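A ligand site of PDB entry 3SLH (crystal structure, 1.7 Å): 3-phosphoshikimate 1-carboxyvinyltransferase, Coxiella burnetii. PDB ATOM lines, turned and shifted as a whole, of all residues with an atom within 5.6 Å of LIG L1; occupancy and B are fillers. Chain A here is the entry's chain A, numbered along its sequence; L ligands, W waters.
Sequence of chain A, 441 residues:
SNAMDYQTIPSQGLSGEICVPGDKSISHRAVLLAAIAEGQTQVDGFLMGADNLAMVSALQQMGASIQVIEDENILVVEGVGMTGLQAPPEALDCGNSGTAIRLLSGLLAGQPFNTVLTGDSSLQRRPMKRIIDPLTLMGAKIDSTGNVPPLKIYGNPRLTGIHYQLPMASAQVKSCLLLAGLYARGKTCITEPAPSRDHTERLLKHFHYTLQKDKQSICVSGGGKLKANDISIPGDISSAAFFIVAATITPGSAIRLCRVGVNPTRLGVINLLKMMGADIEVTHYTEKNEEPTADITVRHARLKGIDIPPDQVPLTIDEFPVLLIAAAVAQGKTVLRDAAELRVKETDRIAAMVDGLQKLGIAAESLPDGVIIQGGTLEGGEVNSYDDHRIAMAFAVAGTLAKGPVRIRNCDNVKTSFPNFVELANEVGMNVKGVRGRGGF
Water W2 lies within hydrogen-bond range of O8 of LIG L1 (2.6 Å), OG of Ser 170 (2.8 Å), NH1 of Arg 130 (2.9 Å) and NH1 of Arg 102 (3.4 Å). Water W5 lies within hydrogen-bond range of O7 of LIG L1 (2.6 Å), O of Ala 169 (3.0 Å) and N of Ala 171 (3.0 Å). Water W4 lies within hydrogen-bond range of O8 of LIG L1, OE1 of Glu 341, NZ of Lys 345 and NH1 of Arg 130. Water W3 lies within hydrogen-bond range of the side-chain hydroxyl (OG1) of Thr 99 (3.0 Å), the side-chain hydroxyl (OG) of Ser 25 (3.2 Å), the side-chain amino group (NZ) of Lys 24 (3.2 Å) and an oxygen (O5) of LIG L1 (3.4 Å).
O6 of LIG L1 sits at hydrogen-bond distance from N of Ala 171, at 3.2 Å. An oxygen (O8) of LIG L1 is in salt-bridge range of the side-chain amino group (NZ) of Lys 345. NH2 of Arg 29 lies within salt-bridge range of O4 of LIG L1 (2.7 Å). NH1 of Arg 102 lies within salt-bridge range of O3 of LG2 L2 (3.7 Å). The guanidinium group (NH1) of Arg 130 is in salt-bridge range of an oxygen (O8) of LIG L1, at 3.9 Å. N of Gln 172 lies within hydrogen-bond range of O6 of LIG L1, 2.8 Å away. An oxygen (O4) of LG2 L2 is in salt-bridge range of the side-chain amino group (NZ) of Lys 24 (2.9 Å). An oxygen (O3) of LG2 L2 is in hydrogen-bond range of the side-chain amide nitrogen of Gln 172 (2.8 Å). The side-chain carboxylate of Asp 318 lies within hydrogen-bond range of an oxygen (O3) of LIG L1 (2.7 Å). OG of Ser 25 is in hydrogen-bond range of O5 of LIG L1, 2.6 Å away. OG of Ser 170 lies within hydrogen-bond range of O6 of LIG L1. The side-chain hydroxyl (OG1) of Thr 99 lies within hydrogen-bond range of an oxygen (O2) of LG2 L2 (2.7 Å). The backbone NH (N) of Thr 99 lies within hydrogen-bond range of an oxygen (O2) of LG2 L2, at 3.2 Å. OE2 of Glu 346 lies within salt-bridge range of N1 of LG2 L2, 2.8 Å away. The guanidinium group of Arg 126 is in salt-bridge range of an oxygen (O3) of LG2 L2, at 2.8 Å. An oxygen (O1) of LIG L1 is in hydrogen-bond range of the side-chain amide nitrogen (NE2) of Gln 172, 3.2 Å away.
OG of Ser 170 sits close to N of Gln 172, 3.3 Å away. The guanidinium group of Arg 29 is in hydrogen-bond range of the side-chain hydroxyl of Ser 175 (3.1 Å). O of Lys 345 sits close to NE of Arg 126. NE2 of Gln 172 lies within hydrogen-bond range of OG1 of Thr 99. The side-chain hydroxyl of Ser 170 sits at hydrogen-bond distance from the backbone NH of Val 173 (3.0 Å). The guanidinium group (NH1) of Arg 29 is in hydrogen-bond range of the backbone carbonyl oxygen (O) of Ser 25. OG of Ser 25 lies within hydrogen-bond range of NH1 of Arg 197 (2.9 Å). NH2 of Arg 197 lies within salt-bridge range of OD2 of Asp 318 (3.7 Å).
O3 of LIG L1 sits at hydrogen-bond distance from N1 of LG2 L2.
Lys 24 touches LIG L1. Thr 99 touches LIG L1 (OG1 to C6, 3.5 Å). Ala 169 touches LIG L1. NH1 of Arg 197 touches C6 of LIG L1, at 3.6 Å. Ile 317 touches LIG L1 (CG2 to O2, 3.99 Å). OE1 of Glu 341 touches O8 of LIG L1, at 3.98 Å. Of the 21 residues printed, 14 come within 4 Å of LIG L1. Along chain A the residues within 4 Å of LIG L1 span positions 24 to 345.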
ATOM      1  N   LYS A  24      -6.048  19.749   7.369  1.00  0.00           N
ATOM      2  CA  LYS A  24      -7.427  19.468   6.904  1.00  0.00           C
ATOM      3  C   LYS A  24      -7.931  20.548   5.928  1.00  0.00           C
ATOM      4  O   LYS A  24      -8.485  20.224   4.868  1.00  0.00           O
ATOM      5  CB  LYS A  24      -8.334  19.346   8.131  1.00  0.00           C
ATOM      6  CG  LYS A  24      -9.781  19.058   7.810  1.00  0.00           C
ATOM      7  CD  LYS A  24     -10.559  18.587   9.034  1.00  0.00           C
ATOM      8  CE  LYS A  24     -10.549  19.564  10.202  1.00  0.00           C
ATOM      9  NZ  LYS A  24     -11.249  20.824   9.940  1.00  0.00           N
ATOM     10  N   SER A  25      -7.690  21.825   6.249  1.00  0.00           N
ATOM     11  CA  SER A  25      -8.165  22.959   5.427  1.00  0.00           C
ATOM     12  C   SER A  25      -7.490  22.972   4.081  1.00  0.00           C
ATOM     13  O   SER A  25      -8.163  23.104   3.026  1.00  0.00           O
ATOM     14  CB  SER A  25      -7.976  24.300   6.131  1.00  0.00           C
ATOM     15  OG  SER A  25      -8.860  24.435   7.212  1.00  0.00           O
ATOM     16  N   ARG A  29      -9.095  22.019  -0.006  1.00  0.00           N
ATOM     17  CA  ARG A  29      -8.909  22.920  -1.141  1.00  0.00           C
ATOM     18  C   ARG A  29      -8.045  22.307  -2.240  1.00  0.00           C
ATOM     19  O   ARG A  29      -8.327  22.482  -3.435  1.00  0.00           O
ATOM     20  CB  ARG A  29      -8.273  24.223  -0.648  1.00  0.00           C
ATOM     21  CG  ARG A  29      -9.209  25.017   0.253  1.00  0.00           C
ATOM     22  CD  ARG A  29      -8.424  25.999   1.077  1.00  0.00           C
ATOM     23  NE  ARG A  29      -9.261  26.965   1.758  1.00  0.00           N
ATOM     24  CZ  ARG A  29      -9.931  26.749   2.891  1.00  0.00           C
ATOM     25  NH1 ARG A  29      -9.924  25.553   3.481  1.00  0.00           N
ATOM     26  NH2 ARG A  29     -10.645  27.743   3.398  1.00  0.00           N
ATOM     27  N   THR A  99     -16.588  22.465   6.214  1.00  0.00           N
ATOM     28  CA  THR A  99     -15.754  22.967   5.142  1.00  0.00           C
ATOM     29  C   THR A  99     -16.148  22.344   3.820  1.00  0.00           C
ATOM     30  O   THR A  99     -16.289  23.024   2.801  1.00  0.00           O
ATOM     31  CB  THR A  99     -14.219  22.697   5.420  1.00  0.00           C
ATOM     32  OG1 THR A  99     -13.855  23.278   6.668  1.00  0.00           O
ATOM     33  CG2 THR A  99     -13.343  23.262   4.281  1.00  0.00           C
ATOM     34  N   ARG A 102     -19.683  23.694   2.610  1.00  0.00           N
ATOM     35  CA  ARG A 102     -19.653  25.094   2.251  1.00  0.00           C
ATOM     36  C   ARG A 102     -18.813  25.362   1.033  1.00  0.00           C
ATOM     37  O   ARG A 102     -19.250  26.133   0.181  1.00  0.00           O
ATOM     38  CB  ARG A 102     -19.299  25.973   3.450  1.00  0.00           C
ATOM     39  CG  ARG A 102     -20.287  25.805   4.596  1.00  0.00           C
ATOM     40  CD  ARG A 102     -20.187  26.942   5.535  1.00  0.00           C
ATOM     41  NE  ARG A 102     -21.040  26.883   6.735  1.00  0.00           N
ATOM     42  CZ  ARG A 102     -20.636  26.552   7.957  1.00  0.00           C
ATOM     43  NH1 ARG A 102     -19.379  26.129   8.194  1.00  0.00           N
ATOM     44  NH2 ARG A 102     -21.488  26.611   8.968  1.00  0.00           N
ATOM     45  N   LEU A 103     -17.629  24.739   0.911  1.00  0.00           N
ATOM     46  CA  LEU A 103     -16.832  24.910  -0.304  1.00  0.00           C
ATOM     47  C   LEU A 103     -17.508  24.260  -1.512  1.00  0.00           C
ATOM     48  O   LEU A 103     -17.559  24.848  -2.576  1.00  0.00           O
ATOM     49  CB  LEU A 103     -15.406  24.410  -0.135  1.00  0.00           C
ATOM     50  CG  LEU A 103     -14.422  25.439   0.461  1.00  0.00           C
ATOM     51  CD1 LEU A 103     -14.863  26.085   1.741  1.00  0.00           C
ATOM     52  CD2 LEU A 103     -13.084  24.749   0.666  1.00  0.00           C
ATOM     53  N   ARG A 126     -25.882  22.825  11.379  1.00  0.00           N
ATOM     54  CA  ARG A 126     -24.993  23.974  11.267  1.00  0.00           C
ATOM     55  C   ARG A 126     -25.405  25.023  10.262  1.00  0.00           C
ATOM     56  O   ARG A 126     -26.078  24.718   9.261  1.00  0.00           O
ATOM     57  CB  ARG A 126     -23.607  23.476  11.147  1.00  0.00           C
ATOM     58  CG  ARG A 126     -23.202  22.884  12.532  1.00  0.00           C
ATOM     59  CD  ARG A 126     -21.859  22.292  12.465  1.00  0.00           C
ATOM     60  NE  ARG A 126     -20.875  23.321  12.195  1.00  0.00           N
ATOM     61  CZ  ARG A 126     -19.716  23.082  11.621  1.00  0.00           C
ATOM     62  NH1 ARG A 126     -19.398  21.857  11.244  1.00  0.00           N
ATOM     63  NH2 ARG A 126     -18.857  24.079  11.385  1.00  0.00           N
ATOM     64  N   ARG A 130     -25.296  31.946   5.812  1.00  0.00           N
ATOM     65  CA  ARG A 130     -24.094  32.708   5.522  1.00  0.00           C
ATOM     66  C   ARG A 130     -23.530  32.502   4.129  1.00  0.00           C
ATOM     67  O   ARG A 130     -22.865  33.392   3.590  1.00  0.00           O
ATOM     68  CB  ARG A 130     -22.997  32.391   6.554  1.00  0.00           C
ATOM     69  CG  ARG A 130     -22.630  30.937   6.624  1.00  0.00           C
ATOM     70  CD  ARG A 130     -21.689  30.624   7.756  1.00  0.00           C
ATOM     71  NE  ARG A 130     -22.220  31.020   9.046  1.00  0.00           N
ATOM     72  CZ  ARG A 130     -21.490  31.151  10.157  1.00  0.00           C
ATOM     73  NH1 ARG A 130     -20.182  30.847  10.142  1.00  0.00           N
ATOM     74  NH2 ARG A 130     -22.060  31.525  11.275  1.00  0.00           N
ATOM     75  N   ALA A 169     -16.352  36.538  10.469  1.00  0.00           N
ATOM     76  CA  ALA A 169     -14.989  36.193  10.074  1.00  0.00           C
ATOM     77  C   ALA A 169     -14.808  34.758   9.602  1.00  0.00           C
ATOM     78  O   ALA A 169     -14.087  33.965  10.233  1.00  0.00           O
ATOM     79  CB  ALA A 169     -14.028  36.462  11.226  1.00  0.00           C
ATOM     80  N   SER A 170     -15.402  34.454   8.445  1.00  0.00           N
ATOM     81  CA  SER A 170     -15.451  33.115   7.906  1.00  0.00           C
ATOM     82  C   SER A 170     -14.652  32.869   6.657  1.00  0.00           C
ATOM     83  O   SER A 170     -14.964  33.389   5.581  1.00  0.00           O
ATOM     84  CB  SER A 170     -16.923  32.768   7.570  1.00  0.00           C
ATOM     85  OG  SER A 170     -16.999  31.451   7.044  1.00  0.00           O
ATOM     86  N   ALA A 171     -13.599  32.080   6.787  1.00  0.00           N
ATOM     87  CA  ALA A 171     -12.786  31.699   5.644  1.00  0.00           C
ATOM     88  C   ALA A 171     -13.627  30.825   4.744  1.00  0.00           C
ATOM     89  O   ALA A 171     -13.410  30.807   3.532  1.00  0.00           O
ATOM     90  CB  ALA A 171     -11.515  30.940   6.087  1.00  0.00           C
ATOM     91  N   GLN A 172     -14.600  30.089   5.316  1.00  0.00           N
ATOM     92  CA  GLN A 172     -15.447  29.238   4.470  1.00  0.00           C
ATOM     93  C   GLN A 172     -16.337  30.048   3.537  1.00  0.00           C
ATOM     94  O   GLN A 172     -16.494  29.688   2.381  1.00  0.00           O
ATOM     95  CB  GLN A 172     -16.259  28.239   5.277  1.00  0.00           C
ATOM     96  CG  GLN A 172     -15.418  27.194   5.947  1.00  0.00           C
ATOM     97  CD  GLN A 172     -16.240  26.188   6.694  1.00  0.00           C
ATOM     98  OE1 GLN A 172     -17.393  25.962   6.342  1.00  0.00           O
ATOM     99  NE2 GLN A 172     -15.677  25.562   7.714  1.00  0.00           N
ATOM    100  N   VAL A 173     -16.925  31.143   4.047  1.00  0.00           N
ATOM    101  CA  VAL A 173     -17.773  31.995   3.217  1.00  0.00           C
ATOM    102  C   VAL A 173     -16.910  32.641   2.158  1.00  0.00           C
ATOM    103  O   VAL A 173     -17.251  32.670   0.972  1.00  0.00           O
ATOM    104  CB  VAL A 173     -18.515  33.037   4.042  1.00  0.00           C
ATOM    105  CG1 VAL A 173     -19.292  33.992   3.149  1.00  0.00           C
ATOM    106  CG2 VAL A 173     -19.476  32.365   5.064  1.00  0.00           C
ATOM    107  N   SER A 175     -14.157  31.529   0.910  1.00  0.00           N
ATOM    108  CA  SER A 175     -13.762  30.480  -0.027  1.00  0.00           C
ATOM    109  C   SER A 175     -14.896  30.046  -0.955  1.00  0.00           C
ATOM    110  O   SER A 175     -14.692  29.899  -2.180  1.00  0.00           O
ATOM    111  CB  SER A 175     -13.203  29.307   0.725  1.00  0.00           C
ATOM    112  OG  SER A 175     -12.075  29.715   1.499  1.00  0.00           O
ATOM    113  N   ARG A 197      -8.224  32.543   7.679  1.00  0.00           N
ATOM    114  CA  ARG A 197      -7.205  31.731   6.963  1.00  0.00           C
ATOM    115  C   ARG A 197      -7.308  31.946   5.451  1.00  0.00           C
ATOM    116  O   ARG A 197      -8.397  32.038   4.898  1.00  0.00           O
ATOM    117  CB  ARG A 197      -7.274  30.258   7.387  1.00  0.00           C
ATOM    118  CG  ARG A 197      -8.507  29.542   6.969  1.00  0.00           C
ATOM    119  CD  ARG A 197      -8.600  28.168   7.647  1.00  0.00           C
ATOM    120  NE  ARG A 197      -8.722  28.335   9.081  1.00  0.00           N
ATOM    121  CZ  ARG A 197      -8.576  27.356   9.968  1.00  0.00           C
ATOM    122  NH1 ARG A 197      -8.349  26.116   9.564  1.00  0.00           N
ATOM    123  NH2 ARG A 197      -8.692  27.628  11.241  1.00  0.00           N
ATOM    124  N   HIS A 199      -5.854  30.118   2.852  1.00  0.00           N
ATOM    125  CA  HIS A 199      -5.399  28.988   2.033  1.00  0.00           C
ATOM    126  C   HIS A 199      -5.992  28.968   0.615  1.00  0.00           C
ATOM    127  O   HIS A 199      -5.318  28.509  -0.317  1.00  0.00           O
ATOM    128  CB  HIS A 199      -5.702  27.652   2.727  1.00  0.00           C
ATOM    129  CG  HIS A 199      -5.213  27.568   4.130  1.00  0.00           C
ATOM    130  ND1 HIS A 199      -3.879  27.682   4.470  1.00  0.00           N
ATOM    131  CD2 HIS A 199      -5.873  27.289   5.286  1.00  0.00           C
ATOM    132  CE1 HIS A 199      -3.748  27.532   5.776  1.00  0.00           C
ATOM    133  NE2 HIS A 199      -4.942  27.303   6.303  1.00  0.00           N
ATOM    134  N   ILE A 317      -9.316  30.148  15.880  1.00  0.00           N
ATOM    135  CA  ILE A 317     -10.684  29.648  16.116  1.00  0.00           C
ATOM    136  C   ILE A 317     -10.823  28.165  16.533  1.00  0.00           C
ATOM    137  O   ILE A 317     -11.518  27.878  17.489  1.00  0.00           O
ATOM    138  CB  ILE A 317     -11.617  30.033  14.930  1.00  0.00           C
ATOM    139  CG1 ILE A 317     -13.085  29.796  15.260  1.00  0.00           C
ATOM    140  CG2 ILE A 317     -11.202  29.334  13.666  1.00  0.00           C
ATOM    141  CD1 ILE A 317     -13.589  30.703  16.401  1.00  0.00           C
ATOM    142  N   ASP A 318     -10.131  27.260  15.846  1.00  0.00           N
ATOM    143  CA  ASP A 318     -10.211  25.850  16.156  1.00  0.00           C
ATOM    144  C   ASP A 318      -9.350  25.423  17.332  1.00  0.00           C
ATOM    145  O   ASP A 318      -9.530  24.317  17.831  1.00  0.00           O
ATOM    146  CB  ASP A 318      -9.854  25.036  14.913  1.00  0.00           C
ATOM    147  CG  ASP A 318     -10.879  25.151  13.815  1.00  0.00           C
ATOM    148  OD1 ASP A 318     -12.018  25.636  14.061  1.00  0.00           O
ATOM    149  OD2 ASP A 318     -10.543  24.719  12.674  1.00  0.00           O
ATOM    150  N   GLU A 341     -18.610  32.657  17.311  1.00  0.00           N
ATOM    151  CA  GLU A 341     -18.531  31.607  16.270  1.00  0.00           C
ATOM    152  C   GLU A 341     -18.288  30.222  16.847  1.00  0.00           C
ATOM    153  O   GLU A 341     -18.600  29.216  16.196  1.00  0.00           O
ATOM    154  CB  GLU A 341     -17.476  31.941  15.229  1.00  0.00           C
ATOM    155  CG  GLU A 341     -17.989  32.911  14.191  1.00  0.00           C
ATOM    156  CD  GLU A 341     -18.929  32.215  13.214  1.00  0.00           C
ATOM    157  OE1 GLU A 341     -18.419  31.384  12.414  1.00  0.00           O
ATOM    158  OE2 GLU A 341     -20.146  32.500  13.263  1.00  0.00           O
ATOM    159  N   LYS A 345     -20.058  25.469  15.807  1.00  0.00           N
ATOM    160  CA  LYS A 345     -19.146  24.475  15.279  1.00  0.00           C
ATOM    161  C   LYS A 345     -19.778  23.075  15.420  1.00  0.00           C
ATOM    162  O   LYS A 345     -21.018  22.963  15.559  1.00  0.00           O
ATOM    163  CB  LYS A 345     -17.785  24.629  15.963  1.00  0.00           C
ATOM    164  CG  LYS A 345     -17.173  26.016  15.711  1.00  0.00           C
ATOM    165  CD  LYS A 345     -16.599  26.150  14.323  1.00  0.00           C
ATOM    166  CE  LYS A 345     -16.120  27.594  14.044  1.00  0.00           C
ATOM    167  NZ  LYS A 345     -15.635  27.745  12.633  1.00  0.00           N
ATOM    168  N   GLU A 346     -18.945  22.028  15.304  1.00  0.00           N
ATOM    169  CA  GLU A 346     -19.404  20.611  15.414  1.00  0.00           C
ATOM    170  C   GLU A 346     -20.337  20.472  16.630  1.00  0.00           C
ATOM    171  O   GLU A 346     -21.349  19.745  16.601  1.00  0.00           O
ATOM    172  CB  GLU A 346     -18.229  19.657  15.480  1.00  0.00           C
ATOM    173  CG  GLU A 346     -17.399  19.512  14.169  1.00  0.00           C
ATOM    174  CD  GLU A 346     -16.307  20.568  13.946  1.00  0.00           C
ATOM    175  OE1 GLU A 346     -16.422  21.721  14.395  1.00  0.00           O
ATOM    176  OE2 GLU A 346     -15.278  20.236  13.299  1.00  0.00           O
HETATM  177  C1  LIG L   1     -11.999  26.479   7.874  1.00  0.00           C
HETATM  178  C2  LIG L   1     -12.545  27.608   8.385  1.00  0.00           C
HETATM  179  C3  LIG L   1     -13.074  27.738   9.788  1.00  0.00           C
HETATM  180  C4  LIG L   1     -12.575  26.563  10.665  1.00  0.00           C
HETATM  181  C5  LIG L   1     -12.652  25.230   9.916  1.00  0.00           C
HETATM  182  C6  LIG L   1     -11.742  25.236   8.697  1.00  0.00           C
HETATM  183  C7  LIG L   1     -11.645  26.443   6.461  1.00  0.00           C
HETATM  184  O1  LIG L   1     -14.528  27.829   9.709  1.00  0.00           O
HETATM  185  O2  LIG L   1     -13.352  26.496  11.860  1.00  0.00           O
HETATM  186  O3  LIG L   1     -12.279  24.087  10.732  1.00  0.00           O
HETATM  187  O4  LIG L   1     -12.010  27.362   5.691  1.00  0.00           O
HETATM  188  O5  LIG L   1     -10.957  25.472   6.049  1.00  0.00           O
HETATM  189  P1  LIG L   1     -15.372  29.222   9.469  1.00  0.00           P
HETATM  190  O6  LIG L   1     -15.142  29.616   8.017  1.00  0.00           O
HETATM  191  O7  LIG L   1     -14.761  30.202  10.473  1.00  0.00           O
HETATM  192  O8  LIG L   1     -16.813  28.858   9.784  1.00  0.00           O
HETATM  193  P1  LG2 L   2     -16.029  22.564   9.838  1.00  0.00           P
HETATM  194  O1  LG2 L   2     -16.791  21.260  10.158  1.00  0.00           O
HETATM  195  O2  LG2 L   2     -14.923  22.165   8.888  1.00  0.00           O
HETATM  196  O3  LG2 L   2     -16.895  23.713   9.463  1.00  0.00           O
HETATM  197  O4  LG2 L   2     -11.837  21.483  12.651  1.00  0.00           O
HETATM  198  O5  LG2 L   2     -11.985  22.360  14.674  1.00  0.00           O
HETATM  199  C1  LG2 L   2     -15.359  23.193  11.376  1.00  0.00           C
HETATM  200  C2  LG2 L   2     -13.698  22.867  13.122  1.00  0.00           C
HETATM  201  C3  LG2 L   2     -12.431  22.154  13.520  1.00  0.00           C
HETATM  202  N1  LG2 L   2     -14.278  22.377  11.885  1.00  0.00           N
HETATM  203  O   HOH W   1     -17.274  26.307  10.470  1.00  0.00           O
HETATM  204  O   HOH W   2     -18.694  29.464   8.121  1.00  0.00           O
HETATM  205  O   HOH W   3     -11.119  22.214   7.067  1.00  0.00           O
HETATM  206  O   HOH W   4     -18.491  28.791  11.825  1.00  0.00           O
HETATM  207  O   HOH W   5     -12.648  31.460   9.609  1.00  0.00           O
